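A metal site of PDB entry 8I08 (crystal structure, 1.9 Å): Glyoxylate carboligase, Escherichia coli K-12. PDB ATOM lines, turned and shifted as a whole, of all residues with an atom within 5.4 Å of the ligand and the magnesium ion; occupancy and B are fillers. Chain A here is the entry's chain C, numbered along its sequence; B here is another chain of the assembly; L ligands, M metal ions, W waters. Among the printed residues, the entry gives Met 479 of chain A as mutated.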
ATOM      1  N   ILE A 394      22.273  16.518  17.554  1.00  0.00           N
ATOM      2  CA  ILE A 394      23.525  17.144  17.127  1.00  0.00           C
ATOM      3  C   ILE A 394      23.181  18.287  16.175  1.00  0.00           C
ATOM      4  O   ILE A 394      22.062  18.393  15.673  1.00  0.00           O
ATOM      5  CB  ILE A 394      24.474  16.122  16.459  1.00  0.00           C
ATOM      6  CG1 ILE A 394      25.927  16.628  16.460  1.00  0.00           C
ATOM      7  CG2 ILE A 394      24.067  15.866  15.028  1.00  0.00           C
ATOM      8  CD1 ILE A 394      26.926  15.577  16.108  1.00  0.00           C
ATOM      9  N   GLY A 395      24.173  19.130  15.896  1.00  0.00           N
ATOM     10  CA  GLY A 395      24.009  20.348  15.134  1.00  0.00           C
ATOM     11  C   GLY A 395      24.437  21.554  15.949  1.00  0.00           C
ATOM     12  O   GLY A 395      24.675  21.478  17.161  1.00  0.00           O
ATOM     13  N   LEU A 396      24.553  22.699  15.256  1.00  0.00           N
ATOM     14  CA  LEU A 396      24.729  23.943  15.993  1.00  0.00           C
ATOM     15  C   LEU A 396      23.544  24.178  16.909  1.00  0.00           C
ATOM     16  O   LEU A 396      23.681  24.757  17.998  1.00  0.00           O
ATOM     17  CB  LEU A 396      24.907  25.124  15.040  1.00  0.00           C
ATOM     18  CG  LEU A 396      26.157  25.158  14.172  1.00  0.00           C
ATOM     19  CD1 LEU A 396      26.252  26.470  13.412  1.00  0.00           C
ATOM     20  CD2 LEU A 396      27.401  24.898  15.004  1.00  0.00           C
ATOM     21  N   SER A 397      22.374  23.678  16.489  1.00  0.00           N
ATOM     22  CA  SER A 397      21.162  23.719  17.295  1.00  0.00           C
ATOM     23  C   SER A 397      21.363  23.058  18.649  1.00  0.00           C
ATOM     24  O   SER A 397      20.918  23.592  19.680  1.00  0.00           O
ATOM     25  CB  SER A 397      20.061  22.980  16.537  1.00  0.00           C
ATOM     26  OG  SER A 397      20.579  21.713  16.101  1.00  0.00           O
ATOM     27  N   ALA A 419      27.342   9.227  19.673  1.00  0.00           N
ATOM     28  CA  ALA A 419      27.103   8.873  18.269  1.00  0.00           C
ATOM     29  C   ALA A 419      26.402   9.968  17.480  1.00  0.00           C
ATOM     30  O   ALA A 419      26.699  10.131  16.284  1.00  0.00           O
ATOM     31  CB  ALA A 419      26.274   7.593  18.195  1.00  0.00           C
ATOM     32  N   GLY A 420      25.482  10.707  18.109  1.00  0.00           N
ATOM     33  CA  GLY A 420      24.709  11.741  17.455  1.00  0.00           C
ATOM     34  C   GLY A 420      24.243  11.454  16.023  1.00  0.00           C
ATOM     35  O   GLY A 420      24.557  12.203  15.106  1.00  0.00           O
ATOM     36  N   PRO A 421      23.503  10.374  15.804  1.00  0.00           N
ATOM     37  CA  PRO A 421      22.906  10.156  14.476  1.00  0.00           C
ATOM     38  C   PRO A 421      21.747  11.102  14.220  1.00  0.00           C
ATOM     39  O   PRO A 421      20.781  11.129  14.982  1.00  0.00           O
ATOM     40  CB  PRO A 421      22.428   8.706  14.531  1.00  0.00           C
ATOM     41  CG  PRO A 421      22.132   8.474  15.970  1.00  0.00           C
ATOM     42  CD  PRO A 421      23.160   9.274  16.730  1.00  0.00           C
ATOM     43  N   LEU A 422      21.799  11.811  13.102  1.00  0.00           N
ATOM     44  CA  LEU A 422      20.697  12.701  12.726  1.00  0.00           C
ATOM     45  C   LEU A 422      19.399  11.919  12.535  1.00  0.00           C
ATOM     46  O   LEU A 422      19.420  10.739  12.151  1.00  0.00           O
ATOM     47  CB  LEU A 422      21.035  13.479  11.444  1.00  0.00           C
ATOM     48  CG  LEU A 422      22.200  14.469  11.495  1.00  0.00           C
ATOM     49  CD1 LEU A 422      22.627  14.825  10.084  1.00  0.00           C
ATOM     50  CD2 LEU A 422      21.840  15.749  12.288  1.00  0.00           C
ATOM     51  N   SER A 445      15.621  20.499  17.454  1.00  0.00           N
ATOM     52  CA  SER A 445      16.281  20.064  16.229  1.00  0.00           C
ATOM     53  C   SER A 445      16.666  21.244  15.355  1.00  0.00           C
ATOM     54  O   SER A 445      15.961  22.262  15.296  1.00  0.00           O
ATOM     55  CB  SER A 445      15.375  19.170  15.375  1.00  0.00           C
ATOM     56  OG  SER A 445      15.099  17.964  16.043  1.00  0.00           O
ATOM     57  N   GLY A 446      17.763  21.063  14.632  1.00  0.00           N
ATOM     58  CA  GLY A 446      17.969  21.839  13.431  1.00  0.00           C
ATOM     59  C   GLY A 446      17.103  21.319  12.303  1.00  0.00           C
ATOM     60  O   GLY A 446      16.446  20.271  12.417  1.00  0.00           O
ATOM     61  N   ASP A 447      17.074  22.075  11.207  1.00  0.00           N
ATOM     62  CA  ASP A 447      16.201  21.701  10.105  1.00  0.00           C
ATOM     63  C   ASP A 447      16.610  20.370   9.475  1.00  0.00           C
ATOM     64  O   ASP A 447      15.743  19.554   9.138  1.00  0.00           O
ATOM     65  CB  ASP A 447      16.123  22.842   9.074  1.00  0.00           C
ATOM     66  CG  ASP A 447      17.491  23.382   8.649  1.00  0.00           C
ATOM     67  OD1 ASP A 447      18.364  23.659   9.508  1.00  0.00           O
ATOM     68  OD2 ASP A 447      17.663  23.552   7.424  1.00  0.00           O
ATOM     69  N   PHE A 448      17.911  20.096   9.385  1.00  0.00           N
ATOM     70  CA  PHE A 448      18.382  18.857   8.733  1.00  0.00           C
ATOM     71  C   PHE A 448      18.106  17.626   9.609  1.00  0.00           C
ATOM     72  O   PHE A 448      17.568  16.614   9.129  1.00  0.00           O
ATOM     73  CB  PHE A 448      19.883  18.988   8.436  1.00  0.00           C
ATOM     74  CG  PHE A 448      20.414  18.035   7.380  1.00  0.00           C
ATOM     75  CD1 PHE A 448      19.763  17.886   6.168  1.00  0.00           C
ATOM     76  CD2 PHE A 448      21.600  17.345   7.587  1.00  0.00           C
ATOM     77  CE1 PHE A 448      20.279  17.018   5.175  1.00  0.00           C
ATOM     78  CE2 PHE A 448      22.127  16.503   6.608  1.00  0.00           C
ATOM     79  CZ  PHE A 448      21.463  16.351   5.398  1.00  0.00           C
ATOM     80  N   ASP A 449      18.433  17.705  10.897  1.00  0.00           N
ATOM     81  CA  ASP A 449      18.074  16.638  11.813  1.00  0.00           C
ATOM     82  C   ASP A 449      16.572  16.387  11.790  1.00  0.00           C
ATOM     83  O   ASP A 449      16.124  15.235  11.824  1.00  0.00           O
ATOM     84  CB  ASP A 449      18.568  17.009  13.218  1.00  0.00           C
ATOM     85  CG  ASP A 449      18.022  16.115  14.303  1.00  0.00           C
ATOM     86  OD1 ASP A 449      18.230  14.883  14.273  1.00  0.00           O
ATOM     87  OD2 ASP A 449      17.389  16.673  15.225  1.00  0.00           O
ATOM     88  N   PHE A 450      15.778  17.451  11.666  1.00  0.00           N
ATOM     89  CA  PHE A 450      14.320  17.328  11.677  1.00  0.00           C
ATOM     90  C   PHE A 450      13.786  16.536  10.489  1.00  0.00           C
ATOM     91  O   PHE A 450      12.748  15.875  10.582  1.00  0.00           O
ATOM     92  CB  PHE A 450      13.702  18.732  11.700  1.00  0.00           C
ATOM     93  CG  PHE A 450      12.235  18.757  12.016  1.00  0.00           C
ATOM     94  CD1 PHE A 450      11.777  18.503  13.306  1.00  0.00           C
ATOM     95  CD2 PHE A 450      11.308  19.092  11.038  1.00  0.00           C
ATOM     96  CE1 PHE A 450      10.432  18.556  13.599  1.00  0.00           C
ATOM     97  CE2 PHE A 450       9.946  19.148  11.327  1.00  0.00           C
ATOM     98  CZ  PHE A 450       9.511  18.880  12.600  1.00  0.00           C
ATOM     99  N   PHE A 452      15.370  14.049   8.595  1.00  0.00           N
ATOM    100  CA  PHE A 452      15.841  12.679   8.382  1.00  0.00           C
ATOM    101  C   PHE A 452      14.729  11.655   8.616  1.00  0.00           C
ATOM    102  O   PHE A 452      14.481  10.769   7.783  1.00  0.00           O
ATOM    103  CB  PHE A 452      16.987  12.371   9.340  1.00  0.00           C
ATOM    104  CG  PHE A 452      18.366  12.467   8.734  1.00  0.00           C
ATOM    105  CD1 PHE A 452      18.840  13.656   8.201  1.00  0.00           C
ATOM    106  CD2 PHE A 452      19.211  11.357   8.759  1.00  0.00           C
ATOM    107  CE1 PHE A 452      20.119  13.727   7.663  1.00  0.00           C
ATOM    108  CE2 PHE A 452      20.492  11.434   8.237  1.00  0.00           C
ATOM    109  CZ  PHE A 452      20.943  12.619   7.696  1.00  0.00           C
ATOM    110  N   VAL A 472      14.695  24.928  14.828  1.00  0.00           N
ATOM    111  CA  VAL A 472      15.484  26.116  14.526  1.00  0.00           C
ATOM    112  C   VAL A 472      15.990  25.951  13.085  1.00  0.00           C
ATOM    113  O   VAL A 472      16.944  25.221  12.816  1.00  0.00           O
ATOM    114  CB  VAL A 472      16.611  26.318  15.549  1.00  0.00           C
ATOM    115  CG1 VAL A 472      16.036  26.800  16.891  1.00  0.00           C
ATOM    116  CG2 VAL A 472      17.402  25.045  15.795  1.00  0.00           C
ATOM    117  N   ASN A 473      15.323  26.635  12.157  1.00  0.00           N
ATOM    118  CA  ASN A 473      15.534  26.462  10.710  1.00  0.00           C
ATOM    119  C   ASN A 473      16.509  27.517  10.204  1.00  0.00           C
ATOM    120  O   ASN A 473      16.156  28.711  10.157  1.00  0.00           O
ATOM    121  CB  ASN A 473      14.203  26.558   9.959  1.00  0.00           C
ATOM    122  CG  ASN A 473      14.347  26.258   8.461  1.00  0.00           C
ATOM    123  OD1 ASN A 473      15.460  26.107   7.941  1.00  0.00           O
ATOM    124  ND2 ASN A 473      13.220  26.157   7.771  1.00  0.00           N
ATOM    125  N   ASN A 474      17.709  27.112   9.796  1.00  0.00           N
ATOM    126  CA  ASN A 474      18.616  28.024   9.102  1.00  0.00           C
ATOM    127  C   ASN A 474      18.833  27.652   7.631  1.00  0.00           C
ATOM    128  O   ASN A 474      19.717  28.226   6.980  1.00  0.00           O
ATOM    129  CB  ASN A 474      19.967  28.123   9.841  1.00  0.00           C
ATOM    130  CG  ASN A 474      20.666  26.776  10.018  1.00  0.00           C
ATOM    131  OD1 ASN A 474      20.329  25.784   9.369  1.00  0.00           O
ATOM    132  ND2 ASN A 474      21.658  26.742  10.926  1.00  0.00           N
ATOM    133  N   ALA A 475      18.049  26.715   7.109  1.00  0.00           N
ATOM    134  CA  ALA A 475      18.190  26.234   5.728  1.00  0.00           C
ATOM    135  C   ALA A 475      19.642  25.874   5.428  1.00  0.00           C
ATOM    136  O   ALA A 475      20.168  26.164   4.353  1.00  0.00           O
ATOM    137  CB  ALA A 475      17.660  27.253   4.729  1.00  0.00           C
ATOM    138  N   TYR A 476      20.289  25.208   6.388  1.00  0.00           N
ATOM    139  CA  TYR A 476      21.722  24.923   6.322  1.00  0.00           C
ATOM    140  C   TYR A 476      22.014  23.663   7.124  1.00  0.00           C
ATOM    141  O   TYR A 476      21.328  23.354   8.102  1.00  0.00           O
ATOM    142  CB  TYR A 476      22.546  26.069   6.922  1.00  0.00           C
ATOM    143  CG  TYR A 476      23.437  26.869   5.994  1.00  0.00           C
ATOM    144  CD1 TYR A 476      24.595  26.325   5.468  1.00  0.00           C
ATOM    145  CD2 TYR A 476      23.152  28.199   5.728  1.00  0.00           C
ATOM    146  CE1 TYR A 476      25.430  27.074   4.651  1.00  0.00           C
ATOM    147  CE2 TYR A 476      23.969  28.962   4.914  1.00  0.00           C
ATOM    148  CZ  TYR A 476      25.117  28.393   4.374  1.00  0.00           C
ATOM    149  OH  TYR A 476      25.942  29.140   3.546  1.00  0.00           O
ATOM    150  N   LEU A 477      23.052  22.942   6.719  1.00  0.00           N
ATOM    151  CA  LEU A 477      23.753  22.052   7.647  1.00  0.00           C
ATOM    152  C   LEU A 477      24.760  22.931   8.392  1.00  0.00           C
ATOM    153  O   LEU A 477      25.974  22.876   8.142  1.00  0.00           O
ATOM    154  CB  LEU A 477      24.447  20.901   6.953  1.00  0.00           C
ATOM    155  CG  LEU A 477      23.967  20.163   5.721  1.00  0.00           C
ATOM    156  CD1 LEU A 477      24.613  18.754   5.685  1.00  0.00           C
ATOM    157  CD2 LEU A 477      22.434  20.121   5.549  1.00  0.00           C
ATOM    158  N   GLY A 478      24.243  23.728   9.325  1.00  0.00           N
ATOM    159  CA  GLY A 478      25.039  24.834   9.845  1.00  0.00           C
ATOM    160  C   GLY A 478      26.297  24.390  10.559  1.00  0.00           C
ATOM    161  O   GLY A 478      27.348  25.019  10.453  1.00  0.00           O
ATOM    162  N   MET A 479      26.220  23.265  11.290  1.00  0.00           N
ATOM    163  CA  MET A 479      27.404  22.763  11.965  1.00  0.00           C
ATOM    164  C   MET A 479      28.508  22.428  10.959  1.00  0.00           C
ATOM    165  O   MET A 479      29.683  22.712  11.217  1.00  0.00           O
ATOM    166  CB  MET A 479      27.046  21.543  12.815  1.00  0.00           C
ATOM    167  CG  MET A 479      28.250  20.833  13.454  1.00  0.00           C
ATOM    168  SD  MET A 479      27.816  19.829  14.892  1.00  0.00           S
ATOM    169  CE  MET A 479      29.338  18.895  15.170  1.00  0.00           C
ATOM    170  N   ILE A 480      28.139  21.869   9.798  1.00  0.00           N
ATOM    171  CA  ILE A 480      29.142  21.474   8.811  1.00  0.00           C
ATOM    172  C   ILE A 480      29.642  22.691   8.049  1.00  0.00           C
ATOM    173  O   ILE A 480      30.820  22.736   7.653  1.00  0.00           O
ATOM    174  CB  ILE A 480      28.601  20.392   7.856  1.00  0.00           C
ATOM    175  CG1 ILE A 480      27.914  19.280   8.652  1.00  0.00           C
ATOM    176  CG2 ILE A 480      29.728  19.787   6.997  1.00  0.00           C
ATOM    177  CD1 ILE A 480      28.758  18.676   9.763  1.00  0.00           C
ATOM    178  N   LEU A 495      20.491  23.988   2.333  1.00  0.00           N
ATOM    179  CA  LEU A 495      19.229  23.304   2.059  1.00  0.00           C
ATOM    180  C   LEU A 495      18.193  24.213   1.421  1.00  0.00           C
ATOM    181  O   LEU A 495      17.070  23.763   1.158  1.00  0.00           O
ATOM    182  CB  LEU A 495      18.656  22.721   3.352  1.00  0.00           C
ATOM    183  CG  LEU A 495      19.481  21.627   4.010  1.00  0.00           C
ATOM    184  CD1 LEU A 495      19.000  21.401   5.415  1.00  0.00           C
ATOM    185  CD2 LEU A 495      19.356  20.355   3.161  1.00  0.00           C
ATOM    186  N   VAL B  26      26.231  13.133   2.286  1.00  0.00           N
ATOM    187  CA  VAL B  26      25.992  14.069   3.382  1.00  0.00           C
ATOM    188  C   VAL B  26      27.356  14.433   3.970  1.00  0.00           C
ATOM    189  O   VAL B  26      28.049  13.554   4.505  1.00  0.00           O
ATOM    190  CB  VAL B  26      25.063  13.478   4.452  1.00  0.00           C
ATOM    191  CG1 VAL B  26      24.927  14.437   5.617  1.00  0.00           C
ATOM    192  CG2 VAL B  26      23.683  13.163   3.878  1.00  0.00           C
ATOM    193  N   PRO B  27      27.778  15.693   3.892  1.00  0.00           N
ATOM    194  CA  PRO B  27      29.072  16.077   4.479  1.00  0.00           C
ATOM    195  C   PRO B  27      29.038  16.082   6.003  1.00  0.00           C
ATOM    196  O   PRO B  27      27.986  16.133   6.647  1.00  0.00           O
ATOM    197  CB  PRO B  27      29.297  17.488   3.918  1.00  0.00           C
ATOM    198  CG  PRO B  27      27.922  18.027   3.773  1.00  0.00           C
ATOM    199  CD  PRO B  27      27.093  16.848   3.303  1.00  0.00           C
ATOM    200  N   GLY B  28      30.237  15.976   6.578  1.00  0.00           N
ATOM    201  CA  GLY B  28      30.451  16.081   8.010  1.00  0.00           C
ATOM    202  C   GLY B  28      31.914  16.397   8.229  1.00  0.00           C
ATOM    203  O   GLY B  28      32.730  16.325   7.312  1.00  0.00           O
ATOM    204  N   VAL B  52      21.265   9.914   5.279  1.00  0.00           N
ATOM    205  CA  VAL B  52      22.402   9.195   4.691  1.00  0.00           C
ATOM    206  C   VAL B  52      21.925   7.934   3.982  1.00  0.00           C
ATOM    207  O   VAL B  52      22.465   7.576   2.926  1.00  0.00           O
ATOM    208  CB  VAL B  52      23.487   8.866   5.732  1.00  0.00           C
ATOM    209  CG1 VAL B  52      24.516   7.891   5.157  1.00  0.00           C
ATOM    210  CG2 VAL B  52      24.203  10.144   6.195  1.00  0.00           C
ATOM    211  N   THR B  76      30.074  10.962   6.562  1.00  0.00           N
ATOM    212  CA  THR B  76      31.079  11.261   7.567  1.00  0.00           C
ATOM    213  C   THR B  76      31.375  10.002   8.393  1.00  0.00           C
ATOM    214  O   THR B  76      31.048   8.878   7.991  1.00  0.00           O
ATOM    215  CB  THR B  76      30.624  12.441   8.438  1.00  0.00           C
ATOM    216  OG1 THR B  76      31.739  12.906   9.204  1.00  0.00           O
ATOM    217  CG2 THR B  76      29.496  12.049   9.397  1.00  0.00           C
ATOM    218  N   PRO B  79      27.888   7.446  12.780  1.00  0.00           N
ATOM    219  CA  PRO B  79      26.530   7.033  12.408  1.00  0.00           C
ATOM    220  C   PRO B  79      26.249   7.037  10.911  1.00  0.00           C
ATOM    221  O   PRO B  79      25.327   6.340  10.461  1.00  0.00           O
ATOM    222  CB  PRO B  79      25.639   8.037  13.170  1.00  0.00           C
ATOM    223  CG  PRO B  79      26.516   9.261  13.315  1.00  0.00           C
ATOM    224  CD  PRO B  79      27.914   8.727  13.506  1.00  0.00           C
ATOM    225  N   ALA B  80      26.971   7.855  10.128  1.00  0.00           N
ATOM    226  CA  ALA B  80      26.774   7.861   8.691  1.00  0.00           C
ATOM    227  C   ALA B  80      27.120   6.515   8.059  1.00  0.00           C
ATOM    228  O   ALA B  80      26.399   6.037   7.174  1.00  0.00           O
ATOM    229  CB  ALA B  80      27.609   8.974   8.059  1.00  0.00           C
ATOM    230  N   ASP B  83      24.375   4.025   8.793  1.00  0.00           N
ATOM    231  CA  ASP B  83      23.187   4.196   7.957  1.00  0.00           C
ATOM    232  C   ASP B  83      23.371   3.685   6.528  1.00  0.00           C
ATOM    233  O   ASP B  83      22.392   3.631   5.781  1.00  0.00           O
ATOM    234  CB  ASP B  83      22.765   5.664   7.882  1.00  0.00           C
ATOM    235  CG  ASP B  83      22.178   6.197   9.186  1.00  0.00           C
ATOM    236  OD1 ASP B  83      21.831   5.376  10.077  1.00  0.00           O
ATOM    237  OD2 ASP B  83      22.058   7.442   9.308  1.00  0.00           O
ATOM    238  N   GLN B 116      32.314  10.087  17.622  1.00  0.00           N
ATOM    239  CA  GLN B 116      31.677   9.538  16.422  1.00  0.00           C
ATOM    240  C   GLN B 116      32.612   8.615  15.638  1.00  0.00           C
ATOM    241  O   GLN B 116      32.610   8.609  14.403  1.00  0.00           O
ATOM    242  CB  GLN B 116      31.134  10.665  15.526  1.00  0.00           C
ATOM    243  CG  GLN B 116      29.788  11.249  15.968  1.00  0.00           C
ATOM    244  CD  GLN B 116      29.222  12.288  14.996  1.00  0.00           C
ATOM    245  OE1 GLN B 116      29.954  13.105  14.435  1.00  0.00           O
ATOM    246  NE2 GLN B 116      27.888  12.263  14.805  1.00  0.00           N
HETATM  247  N1  LIG L   1      25.308  12.051   8.990  1.00  0.00           N
HETATM  248  C1  LIG L   1      24.717  11.567  10.106  1.00  0.00           C
HETATM  249  C2  LIG L   1      23.852  10.357   9.966  1.00  0.00           C
HETATM  250  N2  LIG L   1      24.824  12.101  11.338  1.00  0.00           N
HETATM  251  C3  LIG L   1      25.592  13.188  11.478  1.00  0.00           C
HETATM  252  N3  LIG L   1      25.700  13.692  12.715  1.00  0.00           N
HETATM  253  C4  LIG L   1      26.267  13.781  10.357  1.00  0.00           C
HETATM  254  C5  LIG L   1      26.063  13.141   9.149  1.00  0.00           C
HETATM  255  C6  LIG L   1      27.146  14.994  10.457  1.00  0.00           C
HETATM  256  N4  LIG L   1      26.432  16.210  10.925  1.00  0.00           N
HETATM  257  C7  LIG L   1      26.527  16.699  12.156  1.00  0.00           C
HETATM  258  S1  LIG L   1      25.620  18.099  12.362  1.00  0.00           S
HETATM  259  C8  LIG L   1      25.082  18.041  10.709  1.00  0.00           C
HETATM  260  C9  LIG L   1      25.613  16.976  10.079  1.00  0.00           C
HETATM  261  C10 LIG L   1      25.417  16.578   8.656  1.00  0.00           C
HETATM  262  C11 LIG L   1      24.165  19.095  10.142  1.00  0.00           C
HETATM  263  C12 LIG L   1      23.338  19.795  11.191  1.00  0.00           C
HETATM  264  O1  LIG L   1      22.239  20.453  10.530  1.00  0.00           O
HETATM  265  P1  LIG L   1      20.928  20.923  11.258  1.00  0.00           P
HETATM  266  O2  LIG L   1      20.248  19.726  11.907  1.00  0.00           O
HETATM  267  O3  LIG L   1      20.124  21.729  10.309  1.00  0.00           O
HETATM  268  O4  LIG L   1      21.569  21.877  12.357  1.00  0.00           O
HETATM  269  P2  LIG L   1      22.364  23.251  12.405  1.00  0.00           P
HETATM  270  O5  LIG L   1      22.152  23.968  11.105  1.00  0.00           O
HETATM  271  O6  LIG L   1      21.816  24.019  13.618  1.00  0.00           O
HETATM  272  O7  LIG L   1      23.825  22.854  12.631  1.00  0.00           O
HETATM  273 MG    MG M   1      20.336  23.861  10.105  1.00  0.00          MG
HETATM  274  O   HOH W   1      27.386  12.036   6.701  1.00  0.00           O
HETATM  275  O   HOH W   2      19.941  19.841  14.578  1.00  0.00           O
HETATM  276  O   HOH W   3      19.400  24.433  12.134  1.00  0.00           O
HETATM  277  O   HOH W   4      21.241  26.456  14.544  1.00  0.00           O
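Water W3 lies within hydrogen-bond range of O of Val 472 (2.7 Å), O6 of the ligand (2.9 Å), N of Asp 447 (3.4 Å) and ND2 of Asn 474 (3.4 Å). Water W2 lies within hydrogen-bond range of the side-chain hydroxyl of Ser 397 (2.5 Å), the backbone NH of Gly 446 (2.5 Å), an oxygen (O2) of the ligand (2.7 Å) and the backbone carbonyl oxygen of Ile 394 (2.8 Å). Water W1 lies within hydrogen-bond range of O of Val 26 of chain B (2.8 Å), N of Thr 76 of chain B (2.9 Å) and N1 of the ligand (3.1 Å).
N of Met 479 sits at hydrogen-bond distance from O7 of the ligand (2.8 Å). An oxygen (O2) of the ligand lies within hydrogen-bond range of the backbone NH (N) of Phe 448 (3.5 Å). N of Asp 449 sits at hydrogen-bond distance from O2 of the ligand. N3 of the ligand sits close to NE2 of Gln 116 of chain B, at 3.3 Å. N of Asp 447 lies close to O3 of the ligand (3.2 Å). N of Leu 396 lies within hydrogen-bond range of O7 of the ligand, at 2.7 Å. An oxygen (O7) of the ligand is in hydrogen-bond range of the backbone NH (N) of Gly 478. The backbone carbonyl oxygen of Gly 420 sits at hydrogen-bond distance from a nitrogen (N3) of the ligand (3.0 Å). N of Ser 397 is in hydrogen-bond range of O6 of the ligand (2.9 Å).
Residues that only touch the magnesium ion: Gly 478 (3.99 Å). Four residues have an atom within 4 Å of the magnesium ion: Asp 447, Asn 474, Tyr 476 and Gly 478. The nearest printed residue that does not touch the magnesium ion is Leu 477 (4.4 Å).
The side-chain hydroxyl (OG) of Ser 445 lies within hydrogen-bond range of the side-chain carboxylate (OD2) of Asp 449, 2.8 Å away. The backbone carbonyl oxygen of Gly 420 is in hydrogen-bond range of the side-chain amide nitrogen of Gln 116 of chain B (3.3 Å). The side-chain hydroxyl (OG) of Ser 397 sits at hydrogen-bond distance from the backbone NH (N) of Gly 446, 3.2 Å away. The side-chain carboxylate (OD2) of Asp 447 lies within hydrogen-bond range of the backbone NH (N) of Ala 475 (3.2 Å). The side-chain carboxylate of Asp 447 lies close to the side-chain amide oxygen of Asn 473. The side-chain amide nitrogen (NE2) of Gln 116 of chain B is in hydrogen-bond range of the backbone carbonyl oxygen (O) of Ala 419 (2.9 Å).
Residues that only touch the ligand: Pro 27 of chain B (3.3 Å), Gly 446 (3.5 Å), Asp 83 of chain B (3.5 Å), Leu 422 (3.5 Å), Gly 395 (3.5 Å), Ile 480 (3.6 Å), Val 52 of chain B (3.6 Å), Ile 394 (3.6 Å), Thr 76 of chain B (3.6 Å), Leu 477 (3.6 Å), Val 26 of chain B (3.7 Å), Pro 79 of chain B (3.9 Å), Phe 452 (3.9 Å) and Ala 80 of chain B (3.95 Å). Hydrophobic or aromatic side chains that line the ligand: Ile 394, Leu 396, Leu 422, Phe 448, Phe 452, Leu 477, Met 479, Ile 480, Val 26 of chain B, Val 52 of chain B, Pro 79 of chain B and Ala 80 of chain B. Of the 34 residues printed, 25 come within 4 Å of the ligand.
The side-chain amide oxygen (OD1) of Asn 474 binds the magnesium ion, at 2.1 Å. The side-chain carboxylate (OD1) of Asp 447 is bound to the magnesium ion (2.1 Å). The magnesium ion is bound by O5 of the ligand (2.1 Å). O3 of the ligand is bound to the magnesium ion (2.2 Å). The magnesium ion is bound by O of Tyr 476 (2.3 Å). Water W3 is bound to the magnesium ion (2.3 Å).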
